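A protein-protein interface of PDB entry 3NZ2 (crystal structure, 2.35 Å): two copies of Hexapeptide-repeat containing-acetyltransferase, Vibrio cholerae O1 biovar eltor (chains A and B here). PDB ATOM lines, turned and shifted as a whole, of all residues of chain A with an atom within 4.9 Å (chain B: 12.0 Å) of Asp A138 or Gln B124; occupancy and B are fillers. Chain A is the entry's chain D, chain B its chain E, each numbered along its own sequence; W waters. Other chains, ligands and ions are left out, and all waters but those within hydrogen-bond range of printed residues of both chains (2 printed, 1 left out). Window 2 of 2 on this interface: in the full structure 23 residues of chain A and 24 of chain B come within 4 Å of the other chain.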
ATOM      1  N   ASP A 101      25.975 -26.081   1.991  1.00  0.00           N
ATOM      2  CA  ASP A 101      25.079 -25.000   1.527  1.00  0.00           C
ATOM      3  C   ASP A 101      25.751 -24.057   0.512  1.00  0.00           C
ATOM      4  O   ASP A 101      26.980 -23.909   0.481  1.00  0.00           O
ATOM      5  CB  ASP A 101      24.546 -24.124   2.676  1.00  0.00           C
ATOM      6  CG  ASP A 101      24.030 -24.917   3.850  1.00  0.00           C
ATOM      7  OD1 ASP A 101      23.287 -25.904   3.640  1.00  0.00           O
ATOM      8  OD2 ASP A 101      24.366 -24.530   4.993  1.00  0.00           O
ATOM      9  N   HIS A 102      24.926 -23.430  -0.305  1.00  0.00           N
ATOM     10  CA  HIS A 102      25.388 -22.513  -1.317  1.00  0.00           C
ATOM     11  C   HIS A 102      26.371 -23.192  -2.257  1.00  0.00           C
ATOM     12  O   HIS A 102      27.333 -22.598  -2.688  1.00  0.00           O
ATOM     13  CB  HIS A 102      25.993 -21.283  -0.660  1.00  0.00           C
ATOM     14  CG  HIS A 102      24.990 -20.427   0.041  1.00  0.00           C
ATOM     15  ND1 HIS A 102      24.925 -20.328   1.411  1.00  0.00           N
ATOM     16  CD2 HIS A 102      24.008 -19.632  -0.437  1.00  0.00           C
ATOM     17  CE1 HIS A 102      23.954 -19.500   1.745  1.00  0.00           C
ATOM     18  NE2 HIS A 102      23.381 -19.065   0.642  1.00  0.00           N
ATOM     19  N   VAL A 103      26.110 -24.451  -2.562  1.00  0.00           N
ATOM     20  CA  VAL A 103      26.943 -25.199  -3.489  1.00  0.00           C
ATOM     21  C   VAL A 103      26.349 -25.267  -4.903  1.00  0.00           C
ATOM     22  O   VAL A 103      25.126 -25.427  -5.088  1.00  0.00           O
ATOM     23  CB  VAL A 103      27.149 -26.630  -2.988  1.00  0.00           C
ATOM     24  CG1 VAL A 103      27.857 -27.479  -4.045  1.00  0.00           C
ATOM     25  CG2 VAL A 103      27.915 -26.602  -1.686  1.00  0.00           C
ATOM     26  N   GLU A 136      32.154 -28.952   0.886  1.00  0.00           N
ATOM     27  CA  GLU A 136      31.878 -27.956   1.911  1.00  0.00           C
ATOM     28  C   GLU A 136      31.135 -26.748   1.355  1.00  0.00           C
ATOM     29  O   GLU A 136      30.995 -26.628   0.158  1.00  0.00           O
ATOM     30  CB  GLU A 136      33.176 -27.555   2.606  1.00  0.00           C
ATOM     31  CG  GLU A 136      33.062 -26.380   3.556  1.00  0.00           C
ATOM     32  CD  GLU A 136      32.092 -26.604   4.700  1.00  0.00           C
ATOM     33  OE1 GLU A 136      31.631 -27.745   4.891  1.00  0.00           O
ATOM     34  OE2 GLU A 136      31.796 -25.626   5.413  1.00  0.00           O
ATOM     35  N   ASP A 137      30.616 -25.889   2.229  1.00  0.00           N
ATOM     36  CA  ASP A 137      29.873 -24.689   1.802  1.00  0.00           C
ATOM     37  C   ASP A 137      30.546 -23.826   0.740  1.00  0.00           C
ATOM     38  O   ASP A 137      31.785 -23.682   0.692  1.00  0.00           O
ATOM     39  CB  ASP A 137      29.553 -23.774   2.994  1.00  0.00           C
ATOM     40  CG  ASP A 137      28.725 -24.468   4.081  1.00  0.00           C
ATOM     41  OD1 ASP A 137      27.804 -25.251   3.744  1.00  0.00           O
ATOM     42  OD2 ASP A 137      29.001 -24.221   5.281  1.00  0.00           O
ATOM     43  N   ASP A 138      29.685 -23.254  -0.099  1.00  0.00           N
ATOM     44  CA  ASP A 138      30.040 -22.216  -1.051  1.00  0.00           C
ATOM     45  C   ASP A 138      31.031 -22.665  -2.118  1.00  0.00           C
ATOM     46  O   ASP A 138      31.760 -21.865  -2.688  1.00  0.00           O
ATOM     47  CB  ASP A 138      30.542 -20.963  -0.312  1.00  0.00           C
ATOM     48  CG  ASP A 138      29.401 -20.129   0.269  1.00  0.00           C
ATOM     49  OD1 ASP A 138      28.672 -19.504  -0.536  1.00  0.00           O
ATOM     50  OD2 ASP A 138      29.242 -20.080   1.510  1.00  0.00           O
ATOM     51  N   VAL A 139      31.043 -23.953  -2.394  1.00  0.00           N
ATOM     52  CA  VAL A 139      31.925 -24.485  -3.417  1.00  0.00           C
ATOM     53  C   VAL A 139      31.277 -24.406  -4.808  1.00  0.00           C
ATOM     54  O   VAL A 139      30.045 -24.560  -4.948  1.00  0.00           O
ATOM     55  CB  VAL A 139      32.317 -25.931  -3.062  1.00  0.00           C
ATOM     56  CG1 VAL A 139      33.134 -26.577  -4.196  1.00  0.00           C
ATOM     57  CG2 VAL A 139      33.055 -25.945  -1.701  1.00  0.00           C
ATOM     58  N   TRP A 140      32.092 -24.092  -5.823  1.00  0.00           N
ATOM     59  CA  TRP A 140      31.599 -24.041  -7.209  1.00  0.00           C
ATOM     60  C   TRP A 140      32.288 -25.085  -8.080  1.00  0.00           C
ATOM     61  O   TRP A 140      33.503 -25.026  -8.330  1.00  0.00           O
ATOM     62  CB  TRP A 140      31.709 -22.639  -7.855  1.00  0.00           C
ATOM     63  CG  TRP A 140      31.330 -22.639  -9.341  1.00  0.00           C
ATOM     64  CD1 TRP A 140      30.566 -23.576  -9.994  1.00  0.00           C
ATOM     65  CD2 TRP A 140      31.701 -21.672 -10.341  1.00  0.00           C
ATOM     66  NE1 TRP A 140      30.436 -23.248 -11.325  1.00  0.00           N
ATOM     67  CE2 TRP A 140      31.119 -22.086 -11.564  1.00  0.00           C
ATOM     68  CE3 TRP A 140      32.447 -20.496 -10.323  1.00  0.00           C
ATOM     69  CZ2 TRP A 140      31.288 -21.374 -12.752  1.00  0.00           C
ATOM     70  CZ3 TRP A 140      32.605 -19.791 -11.495  1.00  0.00           C
ATOM     71  CH2 TRP A 140      32.028 -20.233 -12.698  1.00  0.00           C
ATOM     72  N   ARG A 156      34.452 -22.564  -0.214  1.00  0.00           N
ATOM     73  CA  ARG A 156      34.591 -21.344  -1.018  1.00  0.00           C
ATOM     74  C   ARG A 156      35.552 -21.545  -2.176  1.00  0.00           C
ATOM     75  O   ARG A 156      36.098 -20.589  -2.721  1.00  0.00           O
ATOM     76  CB  ARG A 156      35.033 -20.168  -0.141  1.00  0.00           C
ATOM     77  CG  ARG A 156      34.048 -19.912   1.002  1.00  0.00           C
ATOM     78  CD  ARG A 156      34.646 -19.042   2.087  1.00  0.00           C
ATOM     79  NE  ARG A 156      35.906 -19.594   2.564  1.00  0.00           N
ATOM     80  CZ  ARG A 156      36.025 -20.276   3.689  1.00  0.00           C
ATOM     81  NH1 ARG A 156      34.959 -20.464   4.445  1.00  0.00           N
ATOM     82  NH2 ARG A 156      37.200 -20.758   4.057  1.00  0.00           N
ATOM     83  N   SER A 157      35.742 -22.806  -2.546  1.00  0.00           N
ATOM     84  CA  SER A 157      36.644 -23.118  -3.633  1.00  0.00           C
ATOM     85  C   SER A 157      35.914 -23.368  -4.947  1.00  0.00           C
ATOM     86  O   SER A 157      34.709 -23.596  -4.977  1.00  0.00           O
ATOM     87  CB  SER A 157      37.512 -24.298  -3.257  1.00  0.00           C
ATOM     88  OG  SER A 157      38.156 -23.993  -2.035  1.00  0.00           O
ATOM     89  N   HIS B  17      22.495  -9.149 -15.296  1.00  0.00           N
ATOM     90  CA  HIS B  17      21.926  -9.871 -14.161  1.00  0.00           C
ATOM     91  C   HIS B  17      20.398  -9.957 -14.252  1.00  0.00           C
ATOM     92  O   HIS B  17      19.739  -9.026 -14.753  1.00  0.00           O
ATOM     93  CB  HIS B  17      22.388  -9.265 -12.824  1.00  0.00           C
ATOM     94  CG  HIS B  17      23.672  -9.852 -12.308  1.00  0.00           C
ATOM     95  ND1 HIS B  17      24.910  -9.467 -12.773  1.00  0.00           N
ATOM     96  CD2 HIS B  17      23.906 -10.808 -11.375  1.00  0.00           C
ATOM     97  CE1 HIS B  17      25.850 -10.154 -12.148  1.00  0.00           C
ATOM     98  NE2 HIS B  17      25.268 -10.972 -11.292  1.00  0.00           N
ATOM     99  N   PHE B  18      19.854 -11.081 -13.777  1.00  0.00           N
ATOM    100  CA  PHE B  18      18.423 -11.384 -13.909  1.00  0.00           C
ATOM    101  C   PHE B  18      17.903 -12.337 -12.797  1.00  0.00           C
ATOM    102  O   PHE B  18      18.692 -13.027 -12.134  1.00  0.00           O
ATOM    103  CB  PHE B  18      18.164 -12.007 -15.286  1.00  0.00           C
ATOM    104  CG  PHE B  18      18.751 -13.365 -15.430  1.00  0.00           C
ATOM    105  CD1 PHE B  18      17.998 -14.502 -15.115  1.00  0.00           C
ATOM    106  CD2 PHE B  18      20.071 -13.522 -15.811  1.00  0.00           C
ATOM    107  CE1 PHE B  18      18.541 -15.783 -15.239  1.00  0.00           C
ATOM    108  CE2 PHE B  18      20.627 -14.801 -15.937  1.00  0.00           C
ATOM    109  CZ  PHE B  18      19.857 -15.939 -15.636  1.00  0.00           C
ATOM    110  N   ASP B  19      16.580 -12.373 -12.600  1.00  0.00           N
ATOM    111  CA  ASP B  19      15.956 -13.340 -11.675  1.00  0.00           C
ATOM    112  C   ASP B  19      15.383 -14.539 -12.421  1.00  0.00           C
ATOM    113  O   ASP B  19      14.463 -14.404 -13.242  1.00  0.00           O
ATOM    114  CB  ASP B  19      14.852 -12.692 -10.848  1.00  0.00           C
ATOM    115  CG  ASP B  19      14.267 -13.639  -9.807  1.00  0.00           C
ATOM    116  OD1 ASP B  19      14.568 -14.859  -9.836  1.00  0.00           O
ATOM    117  OD2 ASP B  19      13.492 -13.151  -8.955  1.00  0.00           O
ATOM    118  N   GLY B  20      15.923 -15.712 -12.128  1.00  0.00           N
ATOM    119  CA  GLY B  20      15.499 -16.917 -12.806  1.00  0.00           C
ATOM    120  C   GLY B  20      14.077 -17.351 -12.482  1.00  0.00           C
ATOM    121  O   GLY B  20      13.455 -18.063 -13.272  1.00  0.00           O
ATOM    122  N   SER B 115      27.431 -18.771 -16.583  1.00  0.00           N
ATOM    123  CA  SER B 115      28.653 -18.764 -15.804  1.00  0.00           C
ATOM    124  C   SER B 115      28.482 -18.049 -14.478  1.00  0.00           C
ATOM    125  O   SER B 115      27.465 -17.428 -14.230  1.00  0.00           O
ATOM    126  CB  SER B 115      29.818 -18.183 -16.584  1.00  0.00           C
ATOM    127  OG  SER B 115      31.024 -18.757 -16.154  1.00  0.00           O
ATOM    128  N   HIS B 116      29.483 -18.177 -13.620  1.00  0.00           N
ATOM    129  CA  HIS B 116      29.449 -17.579 -12.301  1.00  0.00           C
ATOM    130  C   HIS B 116      30.729 -16.857 -11.927  1.00  0.00           C
ATOM    131  O   HIS B 116      31.776 -17.070 -12.519  1.00  0.00           O
ATOM    132  CB  HIS B 116      29.114 -18.627 -11.248  1.00  0.00           C
ATOM    133  CG  HIS B 116      27.858 -19.377 -11.535  1.00  0.00           C
ATOM    134  ND1 HIS B 116      26.614 -18.803 -11.449  1.00  0.00           N
ATOM    135  CD2 HIS B 116      27.656 -20.649 -11.941  1.00  0.00           C
ATOM    136  CE1 HIS B 116      25.699 -19.692 -11.773  1.00  0.00           C
ATOM    137  NE2 HIS B 116      26.305 -20.819 -12.081  1.00  0.00           N
ATOM    138  N   SER B 117      30.600 -15.964 -10.958  1.00  0.00           N
ATOM    139  CA  SER B 117      31.711 -15.218 -10.411  1.00  0.00           C
ATOM    140  C   SER B 117      32.592 -16.073  -9.521  1.00  0.00           C
ATOM    141  O   SER B 117      32.123 -16.945  -8.813  1.00  0.00           O
ATOM    142  CB  SER B 117      31.207 -14.005  -9.632  1.00  0.00           C
ATOM    143  OG  SER B 117      32.163 -13.546  -8.702  1.00  0.00           O
ATOM    144  N   LEU B 118      33.881 -15.788  -9.557  1.00  0.00           N
ATOM    145  CA  LEU B 118      34.870 -16.453  -8.728  1.00  0.00           C
ATOM    146  C   LEU B 118      34.697 -16.165  -7.233  1.00  0.00           C
ATOM    147  O   LEU B 118      35.140 -16.935  -6.403  1.00  0.00           O
ATOM    148  CB  LEU B 118      36.277 -16.112  -9.197  1.00  0.00           C
ATOM    149  CG  LEU B 118      36.699 -16.890 -10.436  1.00  0.00           C
ATOM    150  CD1 LEU B 118      38.116 -16.593 -10.830  1.00  0.00           C
ATOM    151  CD2 LEU B 118      36.480 -18.364 -10.231  1.00  0.00           C
ATOM    152  N   ASP B 119      34.072 -15.042  -6.904  1.00  0.00           N
ATOM    153  CA  ASP B 119      33.885 -14.652  -5.520  1.00  0.00           C
ATOM    154  C   ASP B 119      32.629 -15.316  -4.963  1.00  0.00           C
ATOM    155  O   ASP B 119      31.521 -15.058  -5.438  1.00  0.00           O
ATOM    156  CB  ASP B 119      33.795 -13.122  -5.388  1.00  0.00           C
ATOM    157  CG  ASP B 119      33.555 -12.676  -3.957  1.00  0.00           C
ATOM    158  OD1 ASP B 119      33.811 -13.463  -3.026  1.00  0.00           O
ATOM    159  OD2 ASP B 119      33.116 -11.536  -3.751  1.00  0.00           O
ATOM    160  N   TYR B 120      32.783 -16.145  -3.942  1.00  0.00           N
ATOM    161  CA  TYR B 120      31.665 -16.885  -3.369  1.00  0.00           C
ATOM    162  C   TYR B 120      30.565 -15.987  -2.822  1.00  0.00           C
ATOM    163  O   TYR B 120      29.411 -16.366  -2.814  1.00  0.00           O
ATOM    164  CB  TYR B 120      32.141 -17.872  -2.307  1.00  0.00           C
ATOM    165  CG  TYR B 120      32.345 -17.249  -0.958  1.00  0.00           C
ATOM    166  CD1 TYR B 120      31.268 -16.965  -0.135  1.00  0.00           C
ATOM    167  CD2 TYR B 120      33.609 -16.932  -0.507  1.00  0.00           C
ATOM    168  CE1 TYR B 120      31.446 -16.384   1.089  1.00  0.00           C
ATOM    169  CE2 TYR B 120      33.790 -16.360   0.717  1.00  0.00           C
ATOM    170  CZ  TYR B 120      32.706 -16.088   1.510  1.00  0.00           C
ATOM    171  OH  TYR B 120      32.892 -15.519   2.732  1.00  0.00           O
ATOM    172  N   ARG B 121      30.928 -14.803  -2.353  1.00  0.00           N
ATOM    173  CA  ARG B 121      29.962 -13.836  -1.836  1.00  0.00           C
ATOM    174  C   ARG B 121      28.998 -13.386  -2.921  1.00  0.00           C
ATOM    175  O   ARG B 121      27.910 -12.929  -2.639  1.00  0.00           O
ATOM    176  CB  ARG B 121      30.663 -12.632  -1.221  1.00  0.00           C
ATOM    177  CG  ARG B 121      31.243 -12.903   0.132  1.00  0.00           C
ATOM    178  CD  ARG B 121      32.691 -12.525   0.186  1.00  0.00           C
ATOM    179  NE  ARG B 121      32.974 -11.363  -0.638  1.00  0.00           N
ATOM    180  CZ  ARG B 121      34.070 -10.626  -0.533  1.00  0.00           C
ATOM    181  NH1 ARG B 121      34.982 -10.932   0.371  1.00  0.00           N
ATOM    182  NH2 ARG B 121      34.254  -9.588  -1.330  1.00  0.00           N
ATOM    183  N   ARG B 122      29.432 -13.483  -4.166  1.00  0.00           N
ATOM    184  CA  ARG B 122      28.609 -13.118  -5.308  1.00  0.00           C
ATOM    185  C   ARG B 122      27.851 -14.282  -5.971  1.00  0.00           C
ATOM    186  O   ARG B 122      27.255 -14.102  -7.010  1.00  0.00           O
ATOM    187  CB  ARG B 122      29.426 -12.326  -6.333  1.00  0.00           C
ATOM    188  CG  ARG B 122      29.843 -10.963  -5.828  1.00  0.00           C
ATOM    189  CD  ARG B 122      30.256 -10.035  -6.946  1.00  0.00           C
ATOM    190  NE  ARG B 122      31.646 -10.234  -7.325  1.00  0.00           N
ATOM    191  CZ  ARG B 122      32.672  -9.565  -6.812  1.00  0.00           C
ATOM    192  NH1 ARG B 122      33.899  -9.830  -7.224  1.00  0.00           N
ATOM    193  NH2 ARG B 122      32.471  -8.640  -5.888  1.00  0.00           N
ATOM    194  N   ARG B 123      27.915 -15.472  -5.386  1.00  0.00           N
ATOM    195  CA  ARG B 123      27.190 -16.638  -5.895  1.00  0.00           C
ATOM    196  C   ARG B 123      26.088 -17.137  -4.969  1.00  0.00           C
ATOM    197  O   ARG B 123      25.437 -18.122  -5.264  1.00  0.00           O
ATOM    198  CB  ARG B 123      28.148 -17.807  -6.108  1.00  0.00           C
ATOM    199  CG  ARG B 123      29.363 -17.532  -6.926  1.00  0.00           C
ATOM    200  CD  ARG B 123      29.946 -18.821  -7.429  1.00  0.00           C
ATOM    201  NE  ARG B 123      30.556 -19.618  -6.379  1.00  0.00           N
ATOM    202  CZ  ARG B 123      31.817 -19.508  -6.000  1.00  0.00           C
ATOM    203  NH1 ARG B 123      32.293 -20.271  -5.047  1.00  0.00           N
ATOM    204  NH2 ARG B 123      32.594 -18.628  -6.568  1.00  0.00           N
ATOM    205  N   GLN B 124      25.894 -16.464  -3.845  1.00  0.00           N
ATOM    206  CA  GLN B 124      25.038 -16.936  -2.794  1.00  0.00           C
ATOM    207  C   GLN B 124      23.556 -16.816  -3.165  1.00  0.00           C
ATOM    208  O   GLN B 124      22.696 -17.477  -2.574  1.00  0.00           O
ATOM    209  CB  GLN B 124      25.394 -16.274  -1.470  1.00  0.00           C
ATOM    210  CG  GLN B 124      25.618 -17.300  -0.411  1.00  0.00           C
ATOM    211  CD  GLN B 124      26.739 -16.970   0.524  1.00  0.00           C
ATOM    212  OE1 GLN B 124      27.277 -15.878   0.498  1.00  0.00           O
ATOM    213  NE2 GLN B 124      27.102 -17.927   1.367  1.00  0.00           N
ATOM    214  N   ALA B 125      23.269 -16.011  -4.182  1.00  0.00           N
ATOM    215  CA  ALA B 125      21.920 -15.943  -4.721  1.00  0.00           C
ATOM    216  C   ALA B 125      21.874 -16.603  -6.104  1.00  0.00           C
ATOM    217  O   ALA B 125      20.998 -16.307  -6.914  1.00  0.00           O
ATOM    218  CB  ALA B 125      21.467 -14.496  -4.798  1.00  0.00           C
ATOM    219  N   TRP B 126      22.848 -17.460  -6.370  1.00  0.00           N
ATOM    220  CA  TRP B 126      22.962 -18.161  -7.639  1.00  0.00           C
ATOM    221  C   TRP B 126      23.080 -17.193  -8.799  1.00  0.00           C
ATOM    222  O   TRP B 126      22.624 -17.484  -9.887  1.00  0.00           O
ATOM    223  CB  TRP B 126      21.762 -19.076  -7.871  1.00  0.00           C
ATOM    224  CG  TRP B 126      21.599 -20.158  -6.874  1.00  0.00           C
ATOM    225  CD1 TRP B 126      22.406 -20.427  -5.834  1.00  0.00           C
ATOM    226  CD2 TRP B 126      20.546 -21.117  -6.825  1.00  0.00           C
ATOM    227  NE1 TRP B 126      21.936 -21.495  -5.137  1.00  0.00           N
ATOM    228  CE2 TRP B 126      20.786 -21.938  -5.726  1.00  0.00           C
ATOM    229  CE3 TRP B 126      19.420 -21.360  -7.610  1.00  0.00           C
ATOM    230  CZ2 TRP B 126      19.946 -22.981  -5.383  1.00  0.00           C
ATOM    231  CZ3 TRP B 126      18.591 -22.401  -7.269  1.00  0.00           C
ATOM    232  CH2 TRP B 126      18.860 -23.198  -6.170  1.00  0.00           C
ATOM    233  N   GLU B 127      23.718 -16.056  -8.575  1.00  0.00           N
ATOM    234  CA  GLU B 127      23.836 -15.045  -9.607  1.00  0.00           C
ATOM    235  C   GLU B 127      24.579 -15.598 -10.818  1.00  0.00           C
ATOM    236  O   GLU B 127      25.642 -16.169 -10.694  1.00  0.00           O
ATOM    237  CB  GLU B 127      24.549 -13.823  -9.036  1.00  0.00           C
ATOM    238  CG  GLU B 127      23.808 -13.139  -7.883  1.00  0.00           C
ATOM    239  CD  GLU B 127      24.302 -13.534  -6.499  1.00  0.00           C
ATOM    240  OE1 GLU B 127      24.488 -14.723  -6.249  1.00  0.00           O
ATOM    241  OE2 GLU B 127      24.497 -12.653  -5.650  1.00  0.00           O
ATOM    242  N   THR B 128      23.991 -15.394 -11.989  1.00  0.00           N
ATOM    243  CA  THR B 128      24.493 -15.929 -13.240  1.00  0.00           C
ATOM    244  C   THR B 128      24.538 -14.912 -14.364  1.00  0.00           C
ATOM    245  O   THR B 128      23.679 -14.057 -14.472  1.00  0.00           O
ATOM    246  CB  THR B 128      23.597 -17.093 -13.753  1.00  0.00           C
ATOM    247  OG1 THR B 128      23.631 -18.183 -12.846  1.00  0.00           O
ATOM    248  CG2 THR B 128      24.063 -17.588 -15.086  1.00  0.00           C
ATOM    249  N   ILE B 129      25.549 -15.038 -15.211  1.00  0.00           N
ATOM    250  CA  ILE B 129      25.652 -14.244 -16.417  1.00  0.00           C
ATOM    251  C   ILE B 129      25.790 -15.178 -17.609  1.00  0.00           C
ATOM    252  O   ILE B 129      26.570 -16.124 -17.573  1.00  0.00           O
ATOM    253  CB  ILE B 129      26.853 -13.304 -16.344  1.00  0.00           C
ATOM    254  CG1 ILE B 129      26.578 -12.195 -15.320  1.00  0.00           C
ATOM    255  CG2 ILE B 129      27.154 -12.742 -17.712  1.00  0.00           C
ATOM    256  CD1 ILE B 129      25.418 -11.265 -15.693  1.00  0.00           C
HETATM  257  O   HOH W   1      25.325 -20.717  -4.218  1.00  0.00           O
HETATM  258  O   HOH W   2      34.981 -18.803  -4.132  1.00  0.00           O
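No position is printed for both chains. Of the 9 pairs that touch across the chains among the printed residues, none has its exchanged pair printed and touching as well.
The backbone carbonyl oxygen of Asp A137 is in hydrogen-bond range of the backbone NH of Arg A156 (3.0 Å). O of Ser A157 sits at hydrogen-bond distance from N of Trp A140, at 2.8 Å. ND1 of His B116 sits at hydrogen-bond distance from O of Glu B127, 2.9 Å away. ND1 of His B116 sits close to OG1 of Thr B128, at 3.4 Å. The side-chain hydroxyl (OG) of Ser B117 is in hydrogen-bond range of the backbone NH (N) of Asp B119 (3.0 Å). O of Leu B118 sits at hydrogen-bond distance from NH2 of Arg B123, at 3.1 Å.
Among the printed residues, merely in contact across the chains: Trp A140 with His B116 (3.0 Å), Arg A156 with Tyr B120 (3.1 Å), Trp A140 with Arg B123 (3.6 Å), Asp A138 with Tyr B120 (3.7 Å), Trp A140 with Ser B117 (3.9 Å) and Trp A140 with Ser B115 (3.9 Å).
Water W2 lies within hydrogen-bond range of O of Arg A156 (2.5 Å), O of Leu B118 (2.9 Å), NH1 of Arg B123 (3.2 Å) and N of Tyr B120 (3.5 Å). Water W1 lies within hydrogen-bond range of O of Arg B123 and O of His A102.
A ring nitrogen (ND1) of His A102 is in hydrogen-bond range of the side-chain amide nitrogen (NE2) of Gln B124 (3.2 Å). NH1 of Arg B123 sits at hydrogen-bond distance from O of Asp A138. The side-chain carboxylate (OD1) of Asp A138 sits at hydrogen-bond distance from the side-chain amide nitrogen (NE2) of Gln B124 (2.9 Å).
Hydrophobic or aromatic side chains of chain B that line the printed part of chain A: His B116 and Tyr B120. Along chain B the printed residues that touch a printed residue of chain A span positions 115 to 124. Hydrophobic or aromatic side chains of chain A that line the printed part of chain B: His A102 and Trp A140.
Of chain A, only His A102 (2.8 Å) and Asp A138 (2.9 Å) come within 4 Å of Gln B124. No residue of chain B comes within 4 Å of Asp A101. No residue of chain B comes within 4 Å of Val A103. Val A139 touches none of the printed residues of chain B. No residue of chain B comes within 4 Å of Ser A157. Printed residues of chain A within 4 Å of Ser B117: Trp A140 (3.9 Å). Printed residues of chain A within 4 Å of Arg B123: Asp A138 and Trp A140. Trp B126 touches none of the printed residues of chain A. The nearest residue of chain B that does not touch Asp A138 is Arg B121 (5.5 Å). The nearest printed residue of chain A that does not touch Gln B124 is Asp A101 (6.0 Å). The nearest printed residue of chain A that does not touch His B116 is Val A139 (8.4 Å).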
